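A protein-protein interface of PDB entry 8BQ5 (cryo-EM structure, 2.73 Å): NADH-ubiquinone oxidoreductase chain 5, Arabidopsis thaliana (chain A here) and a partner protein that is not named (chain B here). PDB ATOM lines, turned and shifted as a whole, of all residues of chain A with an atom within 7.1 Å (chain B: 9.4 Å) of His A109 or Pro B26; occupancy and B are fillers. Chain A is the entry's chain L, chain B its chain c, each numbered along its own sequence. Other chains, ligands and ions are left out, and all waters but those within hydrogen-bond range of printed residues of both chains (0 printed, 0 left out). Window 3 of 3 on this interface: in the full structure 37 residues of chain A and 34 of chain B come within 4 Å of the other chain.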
ATOM      1  N   SER A  25     -25.652   9.273 -29.193  1.00  0.00           N
ATOM      2  CA  SER A  25     -24.539   8.843 -28.354  1.00  0.00           C
ATOM      3  C   SER A  25     -24.500   7.326 -28.224  1.00  0.00           C
ATOM      4  O   SER A  25     -23.432   6.711 -28.317  1.00  0.00           O
ATOM      5  CB  SER A  25     -24.636   9.494 -26.974  1.00  0.00           C
ATOM      6  OG  SER A  25     -24.727  10.902 -27.082  1.00  0.00           O
ATOM      7  N   MET A 104     -16.943   8.877 -21.443  1.00  0.00           N
ATOM      8  CA  MET A 104     -17.550  10.002 -22.141  1.00  0.00           C
ATOM      9  C   MET A 104     -19.072   9.932 -22.133  1.00  0.00           C
ATOM     10  O   MET A 104     -19.715  10.447 -23.053  1.00  0.00           O
ATOM     11  CB  MET A 104     -17.030  10.082 -23.578  1.00  0.00           C
ATOM     12  CG  MET A 104     -15.528  10.295 -23.692  1.00  0.00           C
ATOM     13  SD  MET A 104     -15.010  11.960 -23.234  1.00  0.00           S
ATOM     14  CE  MET A 104     -15.349  12.855 -24.748  1.00  0.00           C
ATOM     15  N   GLU A 106     -21.255  11.418 -20.141  1.00  0.00           N
ATOM     16  CA  GLU A 106     -21.902  12.696 -19.883  1.00  0.00           C
ATOM     17  C   GLU A 106     -21.415  13.815 -20.799  1.00  0.00           C
ATOM     18  O   GLU A 106     -21.833  14.963 -20.620  1.00  0.00           O
ATOM     19  CB  GLU A 106     -21.696  13.099 -18.419  1.00  0.00           C
ATOM     20  CG  GLU A 106     -21.754  11.929 -17.443  1.00  0.00           C
ATOM     21  CD  GLU A 106     -23.165  11.586 -17.007  1.00  0.00           C
ATOM     22  OE1 GLU A 106     -23.767  12.380 -16.253  1.00  0.00           O
ATOM     23  OE2 GLU A 106     -23.671  10.518 -17.411  1.00  0.00           O
ATOM     24  N   ASP A 107     -20.546  13.518 -21.764  1.00  0.00           N
ATOM     25  CA  ASP A 107     -20.075  14.550 -22.679  1.00  0.00           C
ATOM     26  C   ASP A 107     -21.142  14.853 -23.732  1.00  0.00           C
ATOM     27  O   ASP A 107     -21.816  13.938 -24.213  1.00  0.00           O
ATOM     28  CB  ASP A 107     -18.776  14.118 -23.359  1.00  0.00           C
ATOM     29  CG  ASP A 107     -18.089  15.260 -24.092  1.00  0.00           C
ATOM     30  OD1 ASP A 107     -18.515  15.594 -25.218  1.00  0.00           O
ATOM     31  OD2 ASP A 107     -17.129  15.833 -23.538  1.00  0.00           O
ATOM     32  N   PRO A 108     -21.326  16.123 -24.100  1.00  0.00           N
ATOM     33  CA  PRO A 108     -22.323  16.443 -25.133  1.00  0.00           C
ATOM     34  C   PRO A 108     -21.998  15.870 -26.502  1.00  0.00           C
ATOM     35  O   PRO A 108     -22.923  15.582 -27.269  1.00  0.00           O
ATOM     36  CB  PRO A 108     -22.332  17.980 -25.159  1.00  0.00           C
ATOM     37  CG  PRO A 108     -21.655  18.407 -23.905  1.00  0.00           C
ATOM     38  CD  PRO A 108     -20.690  17.330 -23.548  1.00  0.00           C
ATOM     39  N   HIS A 109     -20.722  15.690 -26.832  1.00  0.00           N
ATOM     40  CA  HIS A 109     -20.295  15.385 -28.195  1.00  0.00           C
ATOM     41  C   HIS A 109     -19.589  14.034 -28.293  1.00  0.00           C
ATOM     42  O   HIS A 109     -18.551  13.905 -28.944  1.00  0.00           O
ATOM     43  CB  HIS A 109     -19.396  16.495 -28.724  1.00  0.00           C
ATOM     44  CG  HIS A 109     -20.041  17.844 -28.709  1.00  0.00           C
ATOM     45  ND1 HIS A 109     -19.698  18.824 -27.803  1.00  0.00           N
ATOM     46  CD2 HIS A 109     -21.016  18.373 -29.484  1.00  0.00           C
ATOM     47  CE1 HIS A 109     -20.431  19.899 -28.023  1.00  0.00           C
ATOM     48  NE2 HIS A 109     -21.238  19.653 -29.038  1.00  0.00           N
ATOM     49  N   SER A 110     -20.152  13.014 -27.647  1.00  0.00           N
ATOM     50  CA  SER A 110     -19.577  11.673 -27.734  1.00  0.00           C
ATOM     51  C   SER A 110     -19.543  11.095 -29.146  1.00  0.00           C
ATOM     52  O   SER A 110     -18.515  10.492 -29.502  1.00  0.00           O
ATOM     53  CB  SER A 110     -20.327  10.726 -26.788  1.00  0.00           C
ATOM     54  OG  SER A 110     -20.706  11.393 -25.600  1.00  0.00           O
ATOM     55  N   PRO A 111     -20.594  11.195 -29.976  1.00  0.00           N
ATOM     56  CA  PRO A 111     -20.519  10.552 -31.302  1.00  0.00           C
ATOM     57  C   PRO A 111     -19.366  11.045 -32.156  1.00  0.00           C
ATOM     58  O   PRO A 111     -18.807  10.269 -32.939  1.00  0.00           O
ATOM     59  CB  PRO A 111     -21.876  10.894 -31.932  1.00  0.00           C
ATOM     60  CG  PRO A 111     -22.769  11.137 -30.790  1.00  0.00           C
ATOM     61  CD  PRO A 111     -21.920  11.795 -29.752  1.00  0.00           C
ATOM     62  N   ARG A 112     -18.999  12.322 -32.038  1.00  0.00           N
ATOM     63  CA  ARG A 112     -17.836  12.817 -32.763  1.00  0.00           C
ATOM     64  C   ARG A 112     -16.545  12.303 -32.140  1.00  0.00           C
ATOM     65  O   ARG A 112     -15.567  12.036 -32.847  1.00  0.00           O
ATOM     66  CB  ARG A 112     -17.852  14.344 -32.799  1.00  0.00           C
ATOM     67  CG  ARG A 112     -16.811  14.953 -33.713  1.00  0.00           C
ATOM     68  CD  ARG A 112     -16.907  16.465 -33.718  1.00  0.00           C
ATOM     69  NE  ARG A 112     -16.002  17.075 -32.752  1.00  0.00           N
ATOM     70  CZ  ARG A 112     -16.388  17.688 -31.642  1.00  0.00           C
ATOM     71  NH1 ARG A 112     -17.666  17.797 -31.321  1.00  0.00           N
ATOM     72  NH2 ARG A 112     -15.468  18.205 -30.834  1.00  0.00           N
ATOM     73  N   PHE A 113     -16.524  12.161 -30.814  1.00  0.00           N
ATOM     74  CA  PHE A 113     -15.346  11.621 -30.145  1.00  0.00           C
ATOM     75  C   PHE A 113     -15.076  10.185 -30.579  1.00  0.00           C
ATOM     76  O   PHE A 113     -13.935   9.820 -30.883  1.00  0.00           O
ATOM     77  CB  PHE A 113     -15.521  11.696 -28.631  1.00  0.00           C
ATOM     78  CG  PHE A 113     -14.333  11.206 -27.866  1.00  0.00           C
ATOM     79  CD1 PHE A 113     -13.221  12.012 -27.705  1.00  0.00           C
ATOM     80  CD2 PHE A 113     -14.319   9.934 -27.322  1.00  0.00           C
ATOM     81  CE1 PHE A 113     -12.124  11.562 -27.004  1.00  0.00           C
ATOM     82  CE2 PHE A 113     -13.225   9.479 -26.622  1.00  0.00           C
ATOM     83  CZ  PHE A 113     -12.125  10.293 -26.463  1.00  0.00           C
ATOM     84  N   MET A 114     -16.121   9.354 -30.607  1.00  0.00           N
ATOM     85  CA  MET A 114     -15.960   7.979 -31.068  1.00  0.00           C
ATOM     86  C   MET A 114     -15.558   7.935 -32.534  1.00  0.00           C
ATOM     87  O   MET A 114     -14.799   7.052 -32.948  1.00  0.00           O
ATOM     88  CB  MET A 114     -17.249   7.191 -30.838  1.00  0.00           C
ATOM     89  CG  MET A 114     -17.696   7.147 -29.390  1.00  0.00           C
ATOM     90  SD  MET A 114     -16.339   6.726 -28.282  1.00  0.00           S
ATOM     91  CE  MET A 114     -16.788   5.059 -27.808  1.00  0.00           C
ATOM     92  N   PHE A 153     -10.168  18.397 -28.878  1.00  0.00           N
ATOM     93  CA  PHE A 153     -11.558  17.965 -28.975  1.00  0.00           C
ATOM     94  C   PHE A 153     -12.500  18.959 -28.309  1.00  0.00           C
ATOM     95  O   PHE A 153     -13.585  19.246 -28.828  1.00  0.00           O
ATOM     96  CB  PHE A 153     -11.709  16.579 -28.352  1.00  0.00           C
ATOM     97  CG  PHE A 153     -13.126  16.120 -28.237  1.00  0.00           C
ATOM     98  CD1 PHE A 153     -13.818  15.679 -29.349  1.00  0.00           C
ATOM     99  CD2 PHE A 153     -13.770  16.129 -27.013  1.00  0.00           C
ATOM    100  CE1 PHE A 153     -15.124  15.256 -29.243  1.00  0.00           C
ATOM    101  CE2 PHE A 153     -15.077  15.709 -26.902  1.00  0.00           C
ATOM    102  CZ  PHE A 153     -15.753  15.270 -28.019  1.00  0.00           C
ATOM    103  N   TRP A 154     -12.105  19.495 -27.153  1.00  0.00           N
ATOM    104  CA  TRP A 154     -12.836  20.591 -26.521  1.00  0.00           C
ATOM    105  C   TRP A 154     -12.341  21.895 -27.137  1.00  0.00           C
ATOM    106  O   TRP A 154     -11.483  22.600 -26.600  1.00  0.00           O
ATOM    107  CB  TRP A 154     -12.652  20.560 -25.011  1.00  0.00           C
ATOM    108  CG  TRP A 154     -13.319  19.385 -24.385  1.00  0.00           C
ATOM    109  CD1 TRP A 154     -14.613  18.989 -24.562  1.00  0.00           C
ATOM    110  CD2 TRP A 154     -12.730  18.442 -23.486  1.00  0.00           C
ATOM    111  NE1 TRP A 154     -14.867  17.861 -23.824  1.00  0.00           N
ATOM    112  CE2 TRP A 154     -13.726  17.505 -23.153  1.00  0.00           C
ATOM    113  CE3 TRP A 154     -11.457  18.301 -22.924  1.00  0.00           C
ATOM    114  CZ2 TRP A 154     -13.491  16.441 -22.287  1.00  0.00           C
ATOM    115  CZ3 TRP A 154     -11.226  17.246 -22.064  1.00  0.00           C
ATOM    116  CH2 TRP A 154     -12.236  16.329 -21.754  1.00  0.00           C
ATOM    117  N   PHE A 155     -12.913  22.218 -28.297  1.00  0.00           N
ATOM    118  CA  PHE A 155     -12.382  23.287 -29.133  1.00  0.00           C
ATOM    119  C   PHE A 155     -12.560  24.670 -28.519  1.00  0.00           C
ATOM    120  O   PHE A 155     -11.986  25.637 -29.028  1.00  0.00           O
ATOM    121  CB  PHE A 155     -13.034  23.223 -30.515  1.00  0.00           C
ATOM    122  CG  PHE A 155     -14.526  23.055 -30.476  1.00  0.00           C
ATOM    123  CD1 PHE A 155     -15.349  24.103 -30.107  1.00  0.00           C
ATOM    124  CD2 PHE A 155     -15.104  21.841 -30.805  1.00  0.00           C
ATOM    125  CE1 PHE A 155     -16.718  23.946 -30.069  1.00  0.00           C
ATOM    126  CE2 PHE A 155     -16.476  21.680 -30.770  1.00  0.00           C
ATOM    127  CZ  PHE A 155     -17.282  22.734 -30.402  1.00  0.00           C
ATOM    128  N   GLY B  13     -27.552  23.520 -26.385  1.00  0.00           N
ATOM    129  CA  GLY B  13     -28.012  24.588 -25.517  1.00  0.00           C
ATOM    130  C   GLY B  13     -29.356  25.149 -25.937  1.00  0.00           C
ATOM    131  O   GLY B  13     -30.391  24.513 -25.742  1.00  0.00           O
ATOM    132  N   ASP B  14     -29.342  26.352 -26.509  1.00  0.00           N
ATOM    133  CA  ASP B  14     -30.545  26.983 -27.032  1.00  0.00           C
ATOM    134  C   ASP B  14     -30.510  27.152 -28.543  1.00  0.00           C
ATOM    135  O   ASP B  14     -31.397  26.653 -29.239  1.00  0.00           O
ATOM    136  CB  ASP B  14     -30.756  28.347 -26.360  1.00  0.00           C
ATOM    137  CG  ASP B  14     -31.175  28.223 -24.911  1.00  0.00           C
ATOM    138  OD1 ASP B  14     -31.576  27.114 -24.500  1.00  0.00           O
ATOM    139  OD2 ASP B  14     -31.098  29.231 -24.181  1.00  0.00           O
ATOM    140  N   PHE B  15     -29.499  27.842 -29.075  1.00  0.00           N
ATOM    141  CA  PHE B  15     -29.410  28.003 -30.521  1.00  0.00           C
ATOM    142  C   PHE B  15     -28.933  26.730 -31.206  1.00  0.00           C
ATOM    143  O   PHE B  15     -29.266  26.499 -32.373  1.00  0.00           O
ATOM    144  CB  PHE B  15     -28.500  29.187 -30.875  1.00  0.00           C
ATOM    145  CG  PHE B  15     -27.036  28.935 -30.638  1.00  0.00           C
ATOM    146  CD1 PHE B  15     -26.247  28.339 -31.612  1.00  0.00           C
ATOM    147  CD2 PHE B  15     -26.443  29.316 -29.450  1.00  0.00           C
ATOM    148  CE1 PHE B  15     -24.904  28.114 -31.394  1.00  0.00           C
ATOM    149  CE2 PHE B  15     -25.099  29.097 -29.230  1.00  0.00           C
ATOM    150  CZ  PHE B  15     -24.331  28.494 -30.202  1.00  0.00           C
ATOM    151  N   ARG B  16     -28.167  25.893 -30.502  1.00  0.00           N
ATOM    152  CA  ARG B  16     -27.685  24.653 -31.096  1.00  0.00           C
ATOM    153  C   ARG B  16     -28.820  23.705 -31.458  1.00  0.00           C
ATOM    154  O   ARG B  16     -28.616  22.794 -32.267  1.00  0.00           O
ATOM    155  CB  ARG B  16     -26.696  23.970 -30.150  1.00  0.00           C
ATOM    156  CG  ARG B  16     -25.607  24.902 -29.643  1.00  0.00           C
ATOM    157  CD  ARG B  16     -24.476  24.145 -28.977  1.00  0.00           C
ATOM    158  NE  ARG B  16     -24.819  23.735 -27.621  1.00  0.00           N
ATOM    159  CZ  ARG B  16     -23.945  23.614 -26.633  1.00  0.00           C
ATOM    160  NH1 ARG B  16     -22.661  23.879 -26.809  1.00  0.00           N
ATOM    161  NH2 ARG B  16     -24.372  23.226 -25.434  1.00  0.00           N
ATOM    162  N   ALA B  17     -30.008  23.901 -30.884  1.00  0.00           N
ATOM    163  CA  ALA B  17     -31.182  23.138 -31.285  1.00  0.00           C
ATOM    164  C   ALA B  17     -31.681  23.515 -32.673  1.00  0.00           C
ATOM    165  O   ALA B  17     -32.440  22.745 -33.270  1.00  0.00           O
ATOM    166  CB  ALA B  17     -32.304  23.325 -30.265  1.00  0.00           C
ATOM    167  N   LYS B  18     -31.284  24.673 -33.197  1.00  0.00           N
ATOM    168  CA  LYS B  18     -31.621  25.071 -34.555  1.00  0.00           C
ATOM    169  C   LYS B  18     -30.458  24.884 -35.517  1.00  0.00           C
ATOM    170  O   LYS B  18     -30.489  25.426 -36.626  1.00  0.00           O
ATOM    171  CB  LYS B  18     -32.098  26.526 -34.581  1.00  0.00           C
ATOM    172  CG  LYS B  18     -33.061  26.886 -33.461  1.00  0.00           C
ATOM    173  CD  LYS B  18     -34.124  27.883 -33.920  1.00  0.00           C
ATOM    174  CE  LYS B  18     -33.588  28.886 -34.932  1.00  0.00           C
ATOM    175  NZ  LYS B  18     -32.992  30.080 -34.270  1.00  0.00           N
ATOM    176  N   VAL B  19     -29.436  24.130 -35.122  1.00  0.00           N
ATOM    177  CA  VAL B  19     -28.246  23.916 -35.936  1.00  0.00           C
ATOM    178  C   VAL B  19     -28.221  22.457 -36.366  1.00  0.00           C
ATOM    179  O   VAL B  19     -28.262  21.551 -35.524  1.00  0.00           O
ATOM    180  CB  VAL B  19     -26.964  24.289 -35.178  1.00  0.00           C
ATOM    181  CG1 VAL B  19     -25.744  23.776 -35.921  1.00  0.00           C
ATOM    182  CG2 VAL B  19     -26.884  25.793 -34.979  1.00  0.00           C
ATOM    183  N   TRP B  20     -28.146  22.233 -37.672  1.00  0.00           N
ATOM    184  CA  TRP B  20     -28.071  20.895 -38.240  1.00  0.00           C
ATOM    185  C   TRP B  20     -26.615  20.480 -38.392  1.00  0.00           C
ATOM    186  O   TRP B  20     -25.800  21.241 -38.921  1.00  0.00           O
ATOM    187  CB  TRP B  20     -28.776  20.858 -39.596  1.00  0.00           C
ATOM    188  CG  TRP B  20     -28.981  19.489 -40.166  1.00  0.00           C
ATOM    189  CD1 TRP B  20     -30.111  18.732 -40.089  1.00  0.00           C
ATOM    190  CD2 TRP B  20     -28.036  18.721 -40.926  1.00  0.00           C
ATOM    191  NE1 TRP B  20     -29.928  17.539 -40.743  1.00  0.00           N
ATOM    192  CE2 TRP B  20     -28.663  17.508 -41.266  1.00  0.00           C
ATOM    193  CE3 TRP B  20     -26.721  18.941 -41.347  1.00  0.00           C
ATOM    194  CZ2 TRP B  20     -28.021  16.518 -42.007  1.00  0.00           C
ATOM    195  CZ3 TRP B  20     -26.085  17.958 -42.081  1.00  0.00           C
ATOM    196  CH2 TRP B  20     -26.735  16.761 -42.402  1.00  0.00           C
ATOM    197  N   SER B  21     -26.291  19.277 -37.922  1.00  0.00           N
ATOM    198  CA  SER B  21     -24.972  18.696 -38.123  1.00  0.00           C
ATOM    199  C   SER B  21     -25.130  17.219 -38.453  1.00  0.00           C
ATOM    200  O   SER B  21     -26.150  16.599 -38.144  1.00  0.00           O
ATOM    201  CB  SER B  21     -24.069  18.870 -36.895  1.00  0.00           C
ATOM    202  OG  SER B  21     -24.647  18.281 -35.745  1.00  0.00           O
ATOM    203  N   THR B  23     -23.101  14.828 -37.310  1.00  0.00           N
ATOM    204  CA  THR B  23     -22.770  14.040 -36.133  1.00  0.00           C
ATOM    205  C   THR B  23     -23.844  14.117 -35.056  1.00  0.00           C
ATOM    206  O   THR B  23     -23.782  13.359 -34.083  1.00  0.00           O
ATOM    207  CB  THR B  23     -21.425  14.501 -35.574  1.00  0.00           C
ATOM    208  OG1 THR B  23     -20.579  14.892 -36.660  1.00  0.00           O
ATOM    209  CG2 THR B  23     -20.747  13.373 -34.830  1.00  0.00           C
ATOM    210  N   GLY B  24     -24.826  15.002 -35.210  1.00  0.00           N
ATOM    211  CA  GLY B  24     -25.961  15.063 -34.317  1.00  0.00           C
ATOM    212  C   GLY B  24     -25.984  16.249 -33.381  1.00  0.00           C
ATOM    213  O   GLY B  24     -27.071  16.644 -32.943  1.00  0.00           O
ATOM    214  N   GLY B  25     -24.832  16.831 -33.066  1.00  0.00           N
ATOM    215  CA  GLY B  25     -24.776  17.951 -32.161  1.00  0.00           C
ATOM    216  C   GLY B  25     -24.685  17.518 -30.712  1.00  0.00           C
ATOM    217  O   GLY B  25     -24.491  16.340 -30.401  1.00  0.00           O
ATOM    218  N   PRO B  26     -24.822  18.472 -29.795  1.00  0.00           N
ATOM    219  CA  PRO B  26     -24.706  18.146 -28.370  1.00  0.00           C
ATOM    220  C   PRO B  26     -25.954  17.452 -27.848  1.00  0.00           C
ATOM    221  O   PRO B  26     -27.081  17.895 -28.083  1.00  0.00           O
ATOM    222  CB  PRO B  26     -24.516  19.515 -27.708  1.00  0.00           C
ATOM    223  CG  PRO B  26     -25.164  20.485 -28.644  1.00  0.00           C
ATOM    224  CD  PRO B  26     -25.167  19.886 -30.024  1.00  0.00           C
ATOM    225  N   ASN B  27     -25.732  16.349 -27.129  1.00  0.00           N
ATOM    226  CA  ASN B  27     -26.803  15.572 -26.501  1.00  0.00           C
ATOM    227  C   ASN B  27     -27.801  15.058 -27.538  1.00  0.00           C
ATOM    228  O   ASN B  27     -28.986  15.389 -27.513  1.00  0.00           O
ATOM    229  CB  ASN B  27     -27.515  16.392 -25.423  1.00  0.00           C
ATOM    230  CG  ASN B  27     -26.571  16.896 -24.354  1.00  0.00           C
ATOM    231  OD1 ASN B  27     -25.840  16.122 -23.739  1.00  0.00           O
ATOM    232  ND2 ASN B  27     -26.580  18.205 -24.130  1.00  0.00           N
ATOM    233  N   CYS B  28     -27.312  14.227 -28.454  1.00  0.00           N
ATOM    234  CA  CYS B  28     -28.164  13.663 -29.492  1.00  0.00           C
ATOM    235  C   CYS B  28     -28.828  12.393 -28.973  1.00  0.00           C
ATOM    236  O   CYS B  28     -28.143  11.434 -28.602  1.00  0.00           O
ATOM    237  CB  CYS B  28     -27.353  13.375 -30.752  1.00  0.00           C
ATOM    238  SG  CYS B  28     -28.350  12.973 -32.201  1.00  0.00           S
ATOM    239  N   ARG B  29     -30.159  12.390 -28.940  1.00  0.00           N
ATOM    240  CA  ARG B  29     -30.949  11.252 -28.471  1.00  0.00           C
ATOM    241  C   ARG B  29     -32.091  10.989 -29.444  1.00  0.00           C
ATOM    242  O   ARG B  29     -33.258  11.255 -29.133  1.00  0.00           O
ATOM    243  CB  ARG B  29     -31.497  11.513 -27.068  1.00  0.00           C
ATOM    244  CG  ARG B  29     -30.446  11.739 -25.999  1.00  0.00           C
ATOM    245  CD  ARG B  29     -29.977  10.433 -25.385  1.00  0.00           C
ATOM    246  NE  ARG B  29     -31.076   9.504 -25.152  1.00  0.00           N
ATOM    247  CZ  ARG B  29     -30.982   8.404 -24.417  1.00  0.00           C
ATOM    248  NH1 ARG B  29     -29.864   8.091 -23.782  1.00  0.00           N
ATOM    249  NH2 ARG B  29     -32.036   7.601 -24.310  1.00  0.00           N
ATOM    250  N   PRO B  30     -31.794  10.478 -30.640  1.00  0.00           N
ATOM    251  CA  PRO B  30     -32.871  10.203 -31.599  1.00  0.00           C
ATOM    252  C   PRO B  30     -33.851   9.177 -31.048  1.00  0.00           C
ATOM    253  O   PRO B  30     -33.468   8.232 -30.357  1.00  0.00           O
ATOM    254  CB  PRO B  30     -32.131   9.679 -32.835  1.00  0.00           C
ATOM    255  CG  PRO B  30     -30.786   9.283 -32.352  1.00  0.00           C
ATOM    256  CD  PRO B  30     -30.468  10.163 -31.192  1.00  0.00           C
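The backbone carbonyl oxygen (O) of Cys B28 is in hydrogen-bond range of the backbone NH (N) of Ser A25 (3.4 Å).
The backbone NH of Asn B27 is in hydrogen-bond range of the backbone carbonyl oxygen of Pro A108 (2.9 Å).
The side-chain carboxylate (OD1) of Asp A107 sits at hydrogen-bond distance from the backbone NH (N) of His A109, 2.7 Å away.
The backbone carbonyl oxygen (O) of Phe A153 lies within hydrogen-bond range of the guanidinium group (NH2) of Arg A112, 2.9 Å away.
The side-chain hydroxyl (OG) of Ser B21 lies within hydrogen-bond range of the backbone NH (N) of Gly B25 (3.1 Å).
Among the printed residues, pairs that only touch across the chains: Pro A108 with Gly B25 (3.6 Å), Pro A108 with Pro B26 (3.3 Å), His A109 with Gly B25 (3.96 Å), His A109 with Pro B26 (3.5 Å), Pro A111 with Thr B23 (3.8 Å) and Arg A112 with Thr B23 (3.5 Å).
Printed residues of chain B within 4 Å of Ser A25: Cys B28.
No residue of chain B comes within 4 Å of Ser A110.
Ala B17 touches none of the printed residues of chain A.
Lys B18 touches none of the printed residues of chain A.
Of the printed residues of chain A, Thr B23 touches Pro A111 and Arg A112.
Pro B26 touches just these residues of chain A: Pro A108 and His A109.
The nearest residue of chain B that does not touch His A109 is Arg B16 (4.7 Å).
Of the 14 printed residues of chain A, 5 touch a printed residue of chain B.
Hydrophobic or aromatic side chains of chain A within 4 Å of the printed part of chain B: Pro A108, His A109 and Pro A111.
Along chain A the printed residues that touch a printed residue of chain B span positions 25 to 112.
Printed residues of chain B that touch a printed residue of chain A: Thr B23, Gly B25, Pro B26, Asn B27 and Cys B28.
Among the printed residues, 8 pairs touch across the chains.
Among the printed residues, no Asp or Glu carboxylate lies within 4 Å of a Lys or Arg side-chain nitrogen of the other chain.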
